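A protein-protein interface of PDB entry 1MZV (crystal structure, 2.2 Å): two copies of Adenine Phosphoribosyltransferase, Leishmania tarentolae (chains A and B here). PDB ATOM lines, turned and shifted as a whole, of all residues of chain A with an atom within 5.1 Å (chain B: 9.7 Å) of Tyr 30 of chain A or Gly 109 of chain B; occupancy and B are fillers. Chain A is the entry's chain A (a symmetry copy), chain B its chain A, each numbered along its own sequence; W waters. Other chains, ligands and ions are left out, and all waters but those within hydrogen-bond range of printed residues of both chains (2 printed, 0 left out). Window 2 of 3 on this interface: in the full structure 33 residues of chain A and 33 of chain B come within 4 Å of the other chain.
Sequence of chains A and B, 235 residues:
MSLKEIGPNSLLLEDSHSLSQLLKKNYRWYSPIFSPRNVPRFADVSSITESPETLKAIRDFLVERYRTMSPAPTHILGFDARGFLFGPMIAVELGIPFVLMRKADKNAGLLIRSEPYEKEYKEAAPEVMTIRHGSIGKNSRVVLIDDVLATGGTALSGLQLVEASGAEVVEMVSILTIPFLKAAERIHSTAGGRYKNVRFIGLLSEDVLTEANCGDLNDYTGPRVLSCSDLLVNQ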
ATOM      1  N   ARG A  28       7.729 -32.139  18.462  1.00  0.00           N
ATOM      2  CA  ARG A  28       7.101 -30.951  19.022  1.00  0.00           C
ATOM      3  C   ARG A  28       6.776 -29.988  17.879  1.00  0.00           C
ATOM      4  O   ARG A  28       7.545 -29.846  16.938  1.00  0.00           O
ATOM      5  CB  ARG A  28       8.027 -30.306  20.067  1.00  0.00           C
ATOM      6  CG  ARG A  28       7.318 -29.592  21.198  1.00  0.00           C
ATOM      7  CD  ARG A  28       6.953 -30.472  22.454  1.00  0.00           C
ATOM      8  NE  ARG A  28       6.703 -31.868  22.089  1.00  0.00           N
ATOM      9  CZ  ARG A  28       6.582 -32.887  22.928  1.00  0.00           C
ATOM     10  NH1 ARG A  28       6.647 -32.716  24.242  1.00  0.00           N
ATOM     11  NH2 ARG A  28       6.393 -34.106  22.428  1.00  0.00           N
ATOM     12  N   TRP A  29       5.605 -29.376  17.940  1.00  0.00           N
ATOM     13  CA  TRP A  29       5.185 -28.415  16.942  1.00  0.00           C
ATOM     14  C   TRP A  29       4.715 -27.138  17.626  1.00  0.00           C
ATOM     15  O   TRP A  29       4.327 -27.176  18.783  1.00  0.00           O
ATOM     16  CB  TRP A  29       4.102 -29.025  16.036  1.00  0.00           C
ATOM     17  CG  TRP A  29       2.775 -29.342  16.702  1.00  0.00           C
ATOM     18  CD1 TRP A  29       2.349 -30.562  17.151  1.00  0.00           C
ATOM     19  CD2 TRP A  29       1.707 -28.430  16.951  1.00  0.00           C
ATOM     20  NE1 TRP A  29       1.085 -30.459  17.672  1.00  0.00           N
ATOM     21  CE2 TRP A  29       0.662 -29.161  17.562  1.00  0.00           C
ATOM     22  CE3 TRP A  29       1.519 -27.064  16.722  1.00  0.00           C
ATOM     23  CZ2 TRP A  29      -0.550 -28.571  17.953  1.00  0.00           C
ATOM     24  CZ3 TRP A  29       0.287 -26.477  17.099  1.00  0.00           C
ATOM     25  CH2 TRP A  29      -0.713 -27.232  17.714  1.00  0.00           C
ATOM     26  N   TYR A  30       4.775 -26.016  16.912  1.00  0.00           N
ATOM     27  CA  TYR A  30       4.441 -24.704  17.467  1.00  0.00           C
ATOM     28  C   TYR A  30       3.496 -23.925  16.555  1.00  0.00           C
ATOM     29  O   TYR A  30       3.570 -24.032  15.327  1.00  0.00           O
ATOM     30  CB  TYR A  30       5.720 -23.873  17.686  1.00  0.00           C
ATOM     31  CG  TYR A  30       6.687 -24.445  18.703  1.00  0.00           C
ATOM     32  CD1 TYR A  30       6.666 -24.025  20.028  1.00  0.00           C
ATOM     33  CD2 TYR A  30       7.619 -25.413  18.337  1.00  0.00           C
ATOM     34  CE1 TYR A  30       7.566 -24.543  20.966  1.00  0.00           C
ATOM     35  CE2 TYR A  30       8.523 -25.943  19.267  1.00  0.00           C
ATOM     36  CZ  TYR A  30       8.489 -25.508  20.576  1.00  0.00           C
ATOM     37  OH  TYR A  30       9.360 -26.042  21.488  1.00  0.00           O
ATOM     38  N   SER A  31       2.614 -23.143  17.179  1.00  0.00           N
ATOM     39  CA  SER A  31       1.676 -22.245  16.491  1.00  0.00           C
ATOM     40  C   SER A  31       2.433 -21.038  15.977  1.00  0.00           C
ATOM     41  O   SER A  31       3.574 -20.827  16.395  1.00  0.00           O
ATOM     42  CB  SER A  31       0.607 -21.739  17.465  1.00  0.00           C
ATOM     43  OG  SER A  31      -0.087 -22.813  18.065  1.00  0.00           O
ATOM     44  N   PRO A  32       1.830 -20.260  15.071  1.00  0.00           N
ATOM     45  CA  PRO A  32       2.480 -19.066  14.503  1.00  0.00           C
ATOM     46  C   PRO A  32       3.141 -18.121  15.504  1.00  0.00           C
ATOM     47  O   PRO A  32       4.245 -17.636  15.211  1.00  0.00           O
ATOM     48  CB  PRO A  32       1.329 -18.359  13.780  1.00  0.00           C
ATOM     49  CG  PRO A  32       0.453 -19.486  13.336  1.00  0.00           C
ATOM     50  CD  PRO A  32       0.511 -20.498  14.448  1.00  0.00           C
ATOM     51  N   PHE A  34       4.534 -18.795  18.367  1.00  0.00           N
ATOM     52  CA  PHE A  34       5.767 -19.399  18.900  1.00  0.00           C
ATOM     53  C   PHE A  34       6.669 -19.982  17.797  1.00  0.00           C
ATOM     54  O   PHE A  34       7.473 -20.853  18.076  1.00  0.00           O
ATOM     55  CB  PHE A  34       5.443 -20.516  19.915  1.00  0.00           C
ATOM     56  CG  PHE A  34       5.040 -20.024  21.288  1.00  0.00           C
ATOM     57  CD1 PHE A  34       5.999 -19.617  22.203  1.00  0.00           C
ATOM     58  CD2 PHE A  34       3.696 -20.019  21.676  1.00  0.00           C
ATOM     59  CE1 PHE A  34       5.630 -19.182  23.474  1.00  0.00           C
ATOM     60  CE2 PHE A  34       3.316 -19.584  22.945  1.00  0.00           C
ATOM     61  CZ  PHE A  34       4.278 -19.162  23.847  1.00  0.00           C
ATOM     62  N   SER A  35       6.561 -19.483  16.567  1.00  0.00           N
ATOM     63  CA  SER A  35       7.260 -20.085  15.422  1.00  0.00           C
ATOM     64  C   SER A  35       7.662 -19.049  14.360  1.00  0.00           C
ATOM     65  O   SER A  35       7.145 -17.929  14.340  1.00  0.00           O
ATOM     66  CB  SER A  35       6.405 -21.226  14.799  1.00  0.00           C
ATOM     67  OG  SER A  35       5.881 -20.923  13.510  1.00  0.00           O
ATOM     68  N   VAL A  39       2.368 -21.133   9.338  1.00  0.00           N
ATOM     69  CA  VAL A  39       1.672 -22.410   9.154  1.00  0.00           C
ATOM     70  C   VAL A  39       1.057 -22.797  10.508  1.00  0.00           C
ATOM     71  O   VAL A  39       1.562 -22.382  11.547  1.00  0.00           O
ATOM     72  CB  VAL A  39       2.605 -23.569   8.664  1.00  0.00           C
ATOM     73  CG1 VAL A  39       3.031 -23.371   7.217  1.00  0.00           C
ATOM     74  CG2 VAL A  39       3.834 -23.730   9.554  1.00  0.00           C
ATOM     75  N   PRO A  40      -0.032 -23.569  10.531  1.00  0.00           N
ATOM     76  CA  PRO A  40      -0.718 -23.807  11.806  1.00  0.00           C
ATOM     77  C   PRO A  40       0.094 -24.717  12.722  1.00  0.00           C
ATOM     78  O   PRO A  40       0.031 -24.567  13.945  1.00  0.00           O
ATOM     79  CB  PRO A  40      -2.059 -24.440  11.384  1.00  0.00           C
ATOM     80  CG  PRO A  40      -2.145 -24.216   9.886  1.00  0.00           C
ATOM     81  CD  PRO A  40      -0.720 -24.257   9.421  1.00  0.00           C
ATOM     82  N   ARG A  41       0.857 -25.639  12.149  1.00  0.00           N
ATOM     83  CA  ARG A  41       1.708 -26.489  12.962  1.00  0.00           C
ATOM     84  C   ARG A  41       3.127 -26.543  12.381  1.00  0.00           C
ATOM     85  O   ARG A  41       3.390 -27.164  11.351  1.00  0.00           O
ATOM     86  CB  ARG A  41       1.058 -27.864  13.172  1.00  0.00           C
ATOM     87  CG  ARG A  41      -0.445 -27.736  13.511  1.00  0.00           C
ATOM     88  CD  ARG A  41      -1.014 -28.787  14.416  1.00  0.00           C
ATOM     89  NE  ARG A  41      -0.907 -30.134  13.880  1.00  0.00           N
ATOM     90  CZ  ARG A  41      -1.472 -31.211  14.431  1.00  0.00           C
ATOM     91  NH1 ARG A  41      -2.196 -31.098  15.553  1.00  0.00           N
ATOM     92  NH2 ARG A  41      -1.312 -32.407  13.851  1.00  0.00           N
ATOM     93  N   PHE A  42       4.032 -25.825  13.037  1.00  0.00           N
ATOM     94  CA  PHE A  42       5.435 -25.846  12.646  1.00  0.00           C
ATOM     95  C   PHE A  42       6.130 -26.965  13.412  1.00  0.00           C
ATOM     96  O   PHE A  42       6.301 -26.869  14.614  1.00  0.00           O
ATOM     97  CB  PHE A  42       6.103 -24.497  12.901  1.00  0.00           C
ATOM     98  CG  PHE A  42       7.529 -24.441  12.403  1.00  0.00           C
ATOM     99  CD1 PHE A  42       8.598 -24.766  13.251  1.00  0.00           C
ATOM    100  CD2 PHE A  42       7.797 -24.118  11.077  1.00  0.00           C
ATOM    101  CE1 PHE A  42       9.922 -24.730  12.789  1.00  0.00           C
ATOM    102  CE2 PHE A  42       9.106 -24.093  10.607  1.00  0.00           C
ATOM    103  CZ  PHE A  42      10.186 -24.402  11.477  1.00  0.00           C
ATOM    104  N   ALA A  43       6.495 -28.039  12.713  1.00  0.00           N
ATOM    105  CA  ALA A  43       7.241 -29.162  13.302  1.00  0.00           C
ATOM    106  C   ALA A  43       8.696 -28.805  13.543  1.00  0.00           C
ATOM    107  O   ALA A  43       9.474 -28.655  12.602  1.00  0.00           O
ATOM    108  CB  ALA A  43       7.156 -30.371  12.404  1.00  0.00           C
ATOM    109  N   ASP A  44       9.072 -28.702  14.808  1.00  0.00           N
ATOM    110  CA  ASP A  44      10.399 -28.221  15.190  1.00  0.00           C
ATOM    111  C   ASP A  44      11.390 -29.363  15.113  1.00  0.00           C
ATOM    112  O   ASP A  44      11.309 -30.287  15.901  1.00  0.00           O
ATOM    113  CB  ASP A  44      10.361 -27.691  16.612  1.00  0.00           C
ATOM    114  CG  ASP A  44      11.684 -27.118  17.075  1.00  0.00           C
ATOM    115  OD1 ASP A  44      11.723 -26.742  18.273  1.00  0.00           O
ATOM    116  OD2 ASP A  44      12.718 -26.996  16.350  1.00  0.00           O
ATOM    117  N   GLY A 215       4.375 -27.668  21.575  1.00  0.00           N
ATOM    118  CA  GLY A 215       5.445 -27.094  22.369  1.00  0.00           C
ATOM    119  C   GLY A 215       5.102 -25.745  22.982  1.00  0.00           C
ATOM    120  O   GLY A 215       5.773 -25.333  23.913  1.00  0.00           O
ATOM    121  N   ASP A 216       4.071 -25.073  22.465  1.00  0.00           N
ATOM    122  CA  ASP A 216       3.682 -23.726  22.923  1.00  0.00           C
ATOM    123  C   ASP A 216       3.711 -23.589  24.445  1.00  0.00           C
ATOM    124  O   ASP A 216       3.239 -24.478  25.157  1.00  0.00           O
ATOM    125  CB  ASP A 216       2.265 -23.356  22.443  1.00  0.00           C
ATOM    126  CG  ASP A 216       2.174 -23.136  20.926  1.00  0.00           C
ATOM    127  OD1 ASP A 216       3.176 -23.373  20.224  1.00  0.00           O
ATOM    128  OD2 ASP A 216       1.130 -22.718  20.355  1.00  0.00           O
ATOM    129  N   LYS B 103      19.329 -17.930  13.033  1.00  0.00           N
ATOM    130  CA  LYS B 103      18.651 -16.634  13.042  1.00  0.00           C
ATOM    131  C   LYS B 103      17.238 -16.853  13.626  1.00  0.00           C
ATOM    132  O   LYS B 103      16.679 -17.923  13.493  1.00  0.00           O
ATOM    133  CB  LYS B 103      18.614 -15.985  11.642  1.00  0.00           C
ATOM    134  CG  LYS B 103      19.952 -15.343  11.207  1.00  0.00           C
ATOM    135  CD  LYS B 103      19.814 -14.298  10.090  1.00  0.00           C
ATOM    136  CE  LYS B 103      20.811 -14.505   8.908  1.00  0.00           C
ATOM    137  NZ  LYS B 103      22.235 -14.740   9.327  1.00  0.00           N
ATOM    138  N   ALA B 104      16.723 -15.859  14.338  1.00  0.00           N
ATOM    139  CA  ALA B 104      15.392 -15.901  14.971  1.00  0.00           C
ATOM    140  C   ALA B 104      14.258 -16.335  14.040  1.00  0.00           C
ATOM    141  O   ALA B 104      13.376 -17.080  14.451  1.00  0.00           O
ATOM    142  CB  ALA B 104      15.061 -14.520  15.549  1.00  0.00           C
ATOM    143  N   ASP B 105      14.286 -15.875  12.794  1.00  0.00           N
ATOM    144  CA  ASP B 105      13.242 -16.227  11.827  1.00  0.00           C
ATOM    145  C   ASP B 105      13.432 -17.606  11.174  1.00  0.00           C
ATOM    146  O   ASP B 105      12.761 -17.923  10.188  1.00  0.00           O
ATOM    147  CB  ASP B 105      13.101 -15.140  10.738  1.00  0.00           C
ATOM    148  CG  ASP B 105      14.337 -15.030   9.829  1.00  0.00           C
ATOM    149  OD1 ASP B 105      15.319 -15.750  10.018  1.00  0.00           O
ATOM    150  OD2 ASP B 105      14.413 -14.206   8.897  1.00  0.00           O
ATOM    151  N   LYS B 106      14.357 -18.417  11.693  1.00  0.00           N
ATOM    152  CA  LYS B 106      14.395 -19.829  11.344  1.00  0.00           C
ATOM    153  C   LYS B 106      14.127 -20.712  12.552  1.00  0.00           C
ATOM    154  O   LYS B 106      13.857 -21.906  12.402  1.00  0.00           O
ATOM    155  CB  LYS B 106      15.734 -20.174  10.708  1.00  0.00           C
ATOM    156  CG  LYS B 106      16.021 -19.455   9.396  1.00  0.00           C
ATOM    157  CD  LYS B 106      15.192 -20.031   8.284  1.00  0.00           C
ATOM    158  CE  LYS B 106      15.487 -19.386   6.939  1.00  0.00           C
ATOM    159  NZ  LYS B 106      16.606 -20.119   6.252  1.00  0.00           N
ATOM    160  N   ASN B 107      14.170 -20.141  13.753  1.00  0.00           N
ATOM    161  CA  ASN B 107      14.112 -20.944  14.977  1.00  0.00           C
ATOM    162  C   ASN B 107      12.719 -20.911  15.621  1.00  0.00           C
ATOM    163  O   ASN B 107      12.054 -19.896  15.603  1.00  0.00           O
ATOM    164  CB  ASN B 107      15.188 -20.471  15.970  1.00  0.00           C
ATOM    165  CG  ASN B 107      16.144 -21.586  16.385  1.00  0.00           C
ATOM    166  OD1 ASN B 107      16.033 -22.739  15.914  1.00  0.00           O
ATOM    167  ND2 ASN B 107      17.136 -21.238  17.232  1.00  0.00           N
ATOM    168  N   ALA B 108      12.304 -22.028  16.198  1.00  0.00           N
ATOM    169  CA  ALA B 108      10.987 -22.172  16.819  1.00  0.00           C
ATOM    170  C   ALA B 108      11.027 -22.086  18.339  1.00  0.00           C
ATOM    171  O   ALA B 108      11.996 -22.489  18.972  1.00  0.00           O
ATOM    172  CB  ALA B 108      10.394 -23.514  16.425  1.00  0.00           C
ATOM    173  N   GLY B 109       9.924 -21.621  18.908  1.00  0.00           N
ATOM    174  CA  GLY B 109       9.734 -21.539  20.342  1.00  0.00           C
ATOM    175  C   GLY B 109      10.067 -20.166  20.902  1.00  0.00           C
ATOM    176  O   GLY B 109      10.265 -19.212  20.147  1.00  0.00           O
ATOM    177  N   LEU B 110      10.098 -20.095  22.235  1.00  0.00           N
ATOM    178  CA  LEU B 110      10.628 -18.948  22.989  1.00  0.00           C
ATOM    179  C   LEU B 110      12.147 -18.962  22.820  1.00  0.00           C
ATOM    180  O   LEU B 110      12.788 -19.942  23.175  1.00  0.00           O
ATOM    181  CB  LEU B 110      10.288 -19.095  24.488  1.00  0.00           C
ATOM    182  CG  LEU B 110      10.139 -17.919  25.484  1.00  0.00           C
ATOM    183  CD1 LEU B 110      10.792 -18.270  26.846  1.00  0.00           C
ATOM    184  CD2 LEU B 110      10.673 -16.582  24.984  1.00  0.00           C
ATOM    185  N   LEU B 111      12.703 -17.876  22.284  1.00  0.00           N
ATOM    186  CA  LEU B 111      14.114 -17.789  21.944  1.00  0.00           C
ATOM    187  C   LEU B 111      14.899 -16.817  22.820  1.00  0.00           C
ATOM    188  O   LEU B 111      14.338 -15.938  23.474  1.00  0.00           O
ATOM    189  CB  LEU B 111      14.290 -17.354  20.487  1.00  0.00           C
ATOM    190  CG  LEU B 111      13.426 -18.052  19.420  1.00  0.00           C
ATOM    191  CD1 LEU B 111      13.734 -17.484  18.066  1.00  0.00           C
ATOM    192  CD2 LEU B 111      13.627 -19.575  19.433  1.00  0.00           C
ATOM    193  N   ILE B 112      16.216 -16.999  22.786  1.00  0.00           N
ATOM    194  CA  ILE B 112      17.203 -16.089  23.343  1.00  0.00           C
ATOM    195  C   ILE B 112      18.077 -15.556  22.187  1.00  0.00           C
ATOM    196  O   ILE B 112      18.606 -16.354  21.417  1.00  0.00           O
ATOM    197  CB  ILE B 112      18.110 -16.861  24.352  1.00  0.00           C
ATOM    198  CG1 ILE B 112      17.267 -17.553  25.449  1.00  0.00           C
ATOM    199  CG2 ILE B 112      19.130 -15.914  24.979  1.00  0.00           C
ATOM    200  CD1 ILE B 112      18.081 -18.550  26.350  1.00  0.00           C
ATOM    201  N   ARG B 113      18.246 -14.234  22.061  1.00  0.00           N
ATOM    202  CA  ARG B 113      19.108 -13.683  21.005  1.00  0.00           C
ATOM    203  C   ARG B 113      20.463 -13.185  21.511  1.00  0.00           C
ATOM    204  O   ARG B 113      20.604 -12.728  22.656  1.00  0.00           O
ATOM    205  CB  ARG B 113      18.397 -12.615  20.139  1.00  0.00           C
ATOM    206  CG  ARG B 113      18.140 -11.191  20.720  1.00  0.00           C
ATOM    207  CD  ARG B 113      17.853 -10.158  19.591  1.00  0.00           C
ATOM    208  NE  ARG B 113      17.578  -8.793  20.046  1.00  0.00           N
ATOM    209  CZ  ARG B 113      16.370  -8.254  20.178  1.00  0.00           C
ATOM    210  NH1 ARG B 113      15.262  -8.928  19.866  1.00  0.00           N
ATOM    211  NH2 ARG B 113      16.258  -7.006  20.601  1.00  0.00           N
ATOM    212  N   THR B 130      20.208 -17.085  17.607  1.00  0.00           N
ATOM    213  CA  THR B 130      19.317 -17.476  18.701  1.00  0.00           C
ATOM    214  C   THR B 130      19.453 -18.950  19.053  1.00  0.00           C
ATOM    215  O   THR B 130      19.866 -19.766  18.227  1.00  0.00           O
ATOM    216  CB  THR B 130      17.840 -17.238  18.329  1.00  0.00           C
ATOM    217  OG1 THR B 130      17.467 -18.044  17.198  1.00  0.00           O
ATOM    218  CG2 THR B 130      17.572 -15.784  17.873  1.00  0.00           C
ATOM    219  N   ILE B 131      19.087 -19.297  20.286  1.00  0.00           N
ATOM    220  CA  ILE B 131      18.706 -20.675  20.618  1.00  0.00           C
ATOM    221  C   ILE B 131      17.351 -20.616  21.323  1.00  0.00           C
ATOM    222  O   ILE B 131      16.908 -19.557  21.749  1.00  0.00           O
ATOM    223  CB  ILE B 131      19.796 -21.382  21.511  1.00  0.00           C
ATOM    224  CG1 ILE B 131      19.966 -20.650  22.853  1.00  0.00           C
ATOM    225  CG2 ILE B 131      21.124 -21.455  20.753  1.00  0.00           C
ATOM    226  CD1 ILE B 131      20.784 -21.389  23.892  1.00  0.00           C
ATOM    227  N   ARG B 132      16.694 -21.751  21.462  1.00  0.00           N
ATOM    228  CA  ARG B 132      15.458 -21.791  22.200  1.00  0.00           C
ATOM    229  C   ARG B 132      15.763 -21.759  23.673  1.00  0.00           C
ATOM    230  O   ARG B 132      16.682 -22.437  24.139  1.00  0.00           O
ATOM    231  CB  ARG B 132      14.694 -23.056  21.892  1.00  0.00           C
ATOM    232  CG  ARG B 132      13.266 -23.028  22.428  1.00  0.00           C
ATOM    233  CD  ARG B 132      12.508 -24.293  22.214  1.00  0.00           C
ATOM    234  NE  ARG B 132      13.079 -25.375  23.013  1.00  0.00           N
ATOM    235  CZ  ARG B 132      13.979 -26.263  22.604  1.00  0.00           C
ATOM    236  NH1 ARG B 132      14.478 -26.234  21.379  1.00  0.00           N
ATOM    237  NH2 ARG B 132      14.409 -27.180  23.448  1.00  0.00           N
ATOM    238  N   HIS B 133      14.964 -20.997  24.408  1.00  0.00           N
ATOM    239  CA  HIS B 133      15.152 -20.850  25.836  1.00  0.00           C
ATOM    240  C   HIS B 133      14.895 -22.193  26.468  1.00  0.00           C
ATOM    241  O   HIS B 133      13.854 -22.802  26.251  1.00  0.00           O
ATOM    242  CB  HIS B 133      14.201 -19.807  26.401  1.00  0.00           C
ATOM    243  CG  HIS B 133      14.279 -19.653  27.891  1.00  0.00           C
ATOM    244  ND1 HIS B 133      14.960 -18.617  28.501  1.00  0.00           N
ATOM    245  CD2 HIS B 133      13.750 -20.394  28.895  1.00  0.00           C
ATOM    246  CE1 HIS B 133      14.838 -18.722  29.814  1.00  0.00           C
ATOM    247  NE2 HIS B 133      14.123 -19.801  30.081  1.00  0.00           N
ATOM    248  N   GLY B 134      15.877 -22.665  27.220  1.00  0.00           N
ATOM    249  CA  GLY B 134      15.774 -23.928  27.910  1.00  0.00           C
ATOM    250  C   GLY B 134      16.301 -25.093  27.114  1.00  0.00           C
ATOM    251  O   GLY B 134      16.274 -26.217  27.604  1.00  0.00           O
ATOM    252  N   SER B 135      16.779 -24.839  25.898  1.00  0.00           N
ATOM    253  CA  SER B 135      17.388 -25.899  25.087  1.00  0.00           C
ATOM    254  C   SER B 135      18.688 -26.375  25.722  1.00  0.00           C
ATOM    255  O   SER B 135      19.083 -27.549  25.594  1.00  0.00           O
ATOM    256  CB  SER B 135      17.643 -25.426  23.649  1.00  0.00           C
ATOM    257  OG  SER B 135      18.530 -24.327  23.585  1.00  0.00           O
HETATM  258  O   HOH W   1      13.751 -24.664  15.455  1.00  0.00           O
HETATM  259  O   HOH W   2      13.384 -25.038  18.916  1.00  0.00           O
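The backbone NH (N) of Gly 109 of chain B lies within hydrogen-bond range of the backbone carbonyl oxygen (O) of Phe 34 of chain A, at 2.7 Å.
The backbone carbonyl oxygen of Arg 132 of chain B is in hydrogen-bond range of the side-chain hydroxyl of Ser 135 of chain B (2.7 Å).
N of Tyr 30 of chain A sits at hydrogen-bond distance from O of Phe 42 of chain A, 2.9 Å away.
The backbone carbonyl oxygen (O) of Arg 28 of chain A is in hydrogen-bond range of the backbone NH (N) of Asp 44 of chain A (2.9 Å).
Among the printed residues, merely in contact across the chains: Tyr 30 of chain A with Arg 132 of chain B (3.7 Å), Tyr 30 of chain A with Gly 109 of chain B (3.8 Å), Phe 34 of chain A with Ala 108 of chain B (3.8 Å), Phe 42 of chain A with Ala 108 of chain B (3.9 Å), Tyr 30 of chain A with Ala 108 of chain B (3.9 Å) and Asp 44 of chain A with Ala 108 of chain B (3.9 Å).
Of chain B, only Ala 108, Gly 109 and Arg 132 come within 4 Å of Tyr 30 of chain A.
No residue of chain B comes within 4 Å of Ser 31 of chain A.
Printed residues of chain B within 4 Å of Phe 34 of chain A: Ala 108 and Gly 109.
Arg 41 of chain A touches none of the printed residues of chain B.
Printed residues of chain B within 4 Å of Asp 44 of chain A: Ala 108 (3.9 Å).
No residue of chain B comes within 4 Å of Gly 215 of chain A.
Of the printed residues of chain A, Ala 108 of chain B touches Tyr 30, Phe 34, Phe 42 and Asp 44.
Gly 109 of chain B touches just these residues of chain A: Tyr 30 and Phe 34.
Printed residues of chain A within 4 Å of Arg 132 of chain B: Tyr 30 (3.7 Å).
Ser 135 of chain B touches none of the printed residues of chain A.
The nearest residue of chain B that does not touch Tyr 30 of chain A is Leu 110 of chain B (5.3 Å).
Of the 17 printed residues of chain B, 3 touch a printed residue of chain A.
Hydrophobic or aromatic side chains of chain B that line the printed part of chain A: Ala 108.
Among the printed residues, 7 pairs touch across the chains.
Among the printed residues, no Asp or Glu carboxylate lies within 4 Å of a Lys or Arg side-chain nitrogen of the other chain.
No position is printed for both chains.
Of the 7 pairs that touch across the chains among the printed residues, none has its exchanged pair printed and touching as well.
Water W2 lies within hydrogen-bond range of the side-chain carboxylate (OD1) of Asp 44 of chain A, the backbone carbonyl oxygen (O) of Ala 108 of chain B and the guanidinium group (NH1) of Arg 132 of chain B.
Water W1 lies within hydrogen-bond range of OD2 of Asp 44 of chain A (2.7 Å), OD1 of Asn 107 of chain B (3.0 Å) and N of Ala 108 of chain B (3.1 Å).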
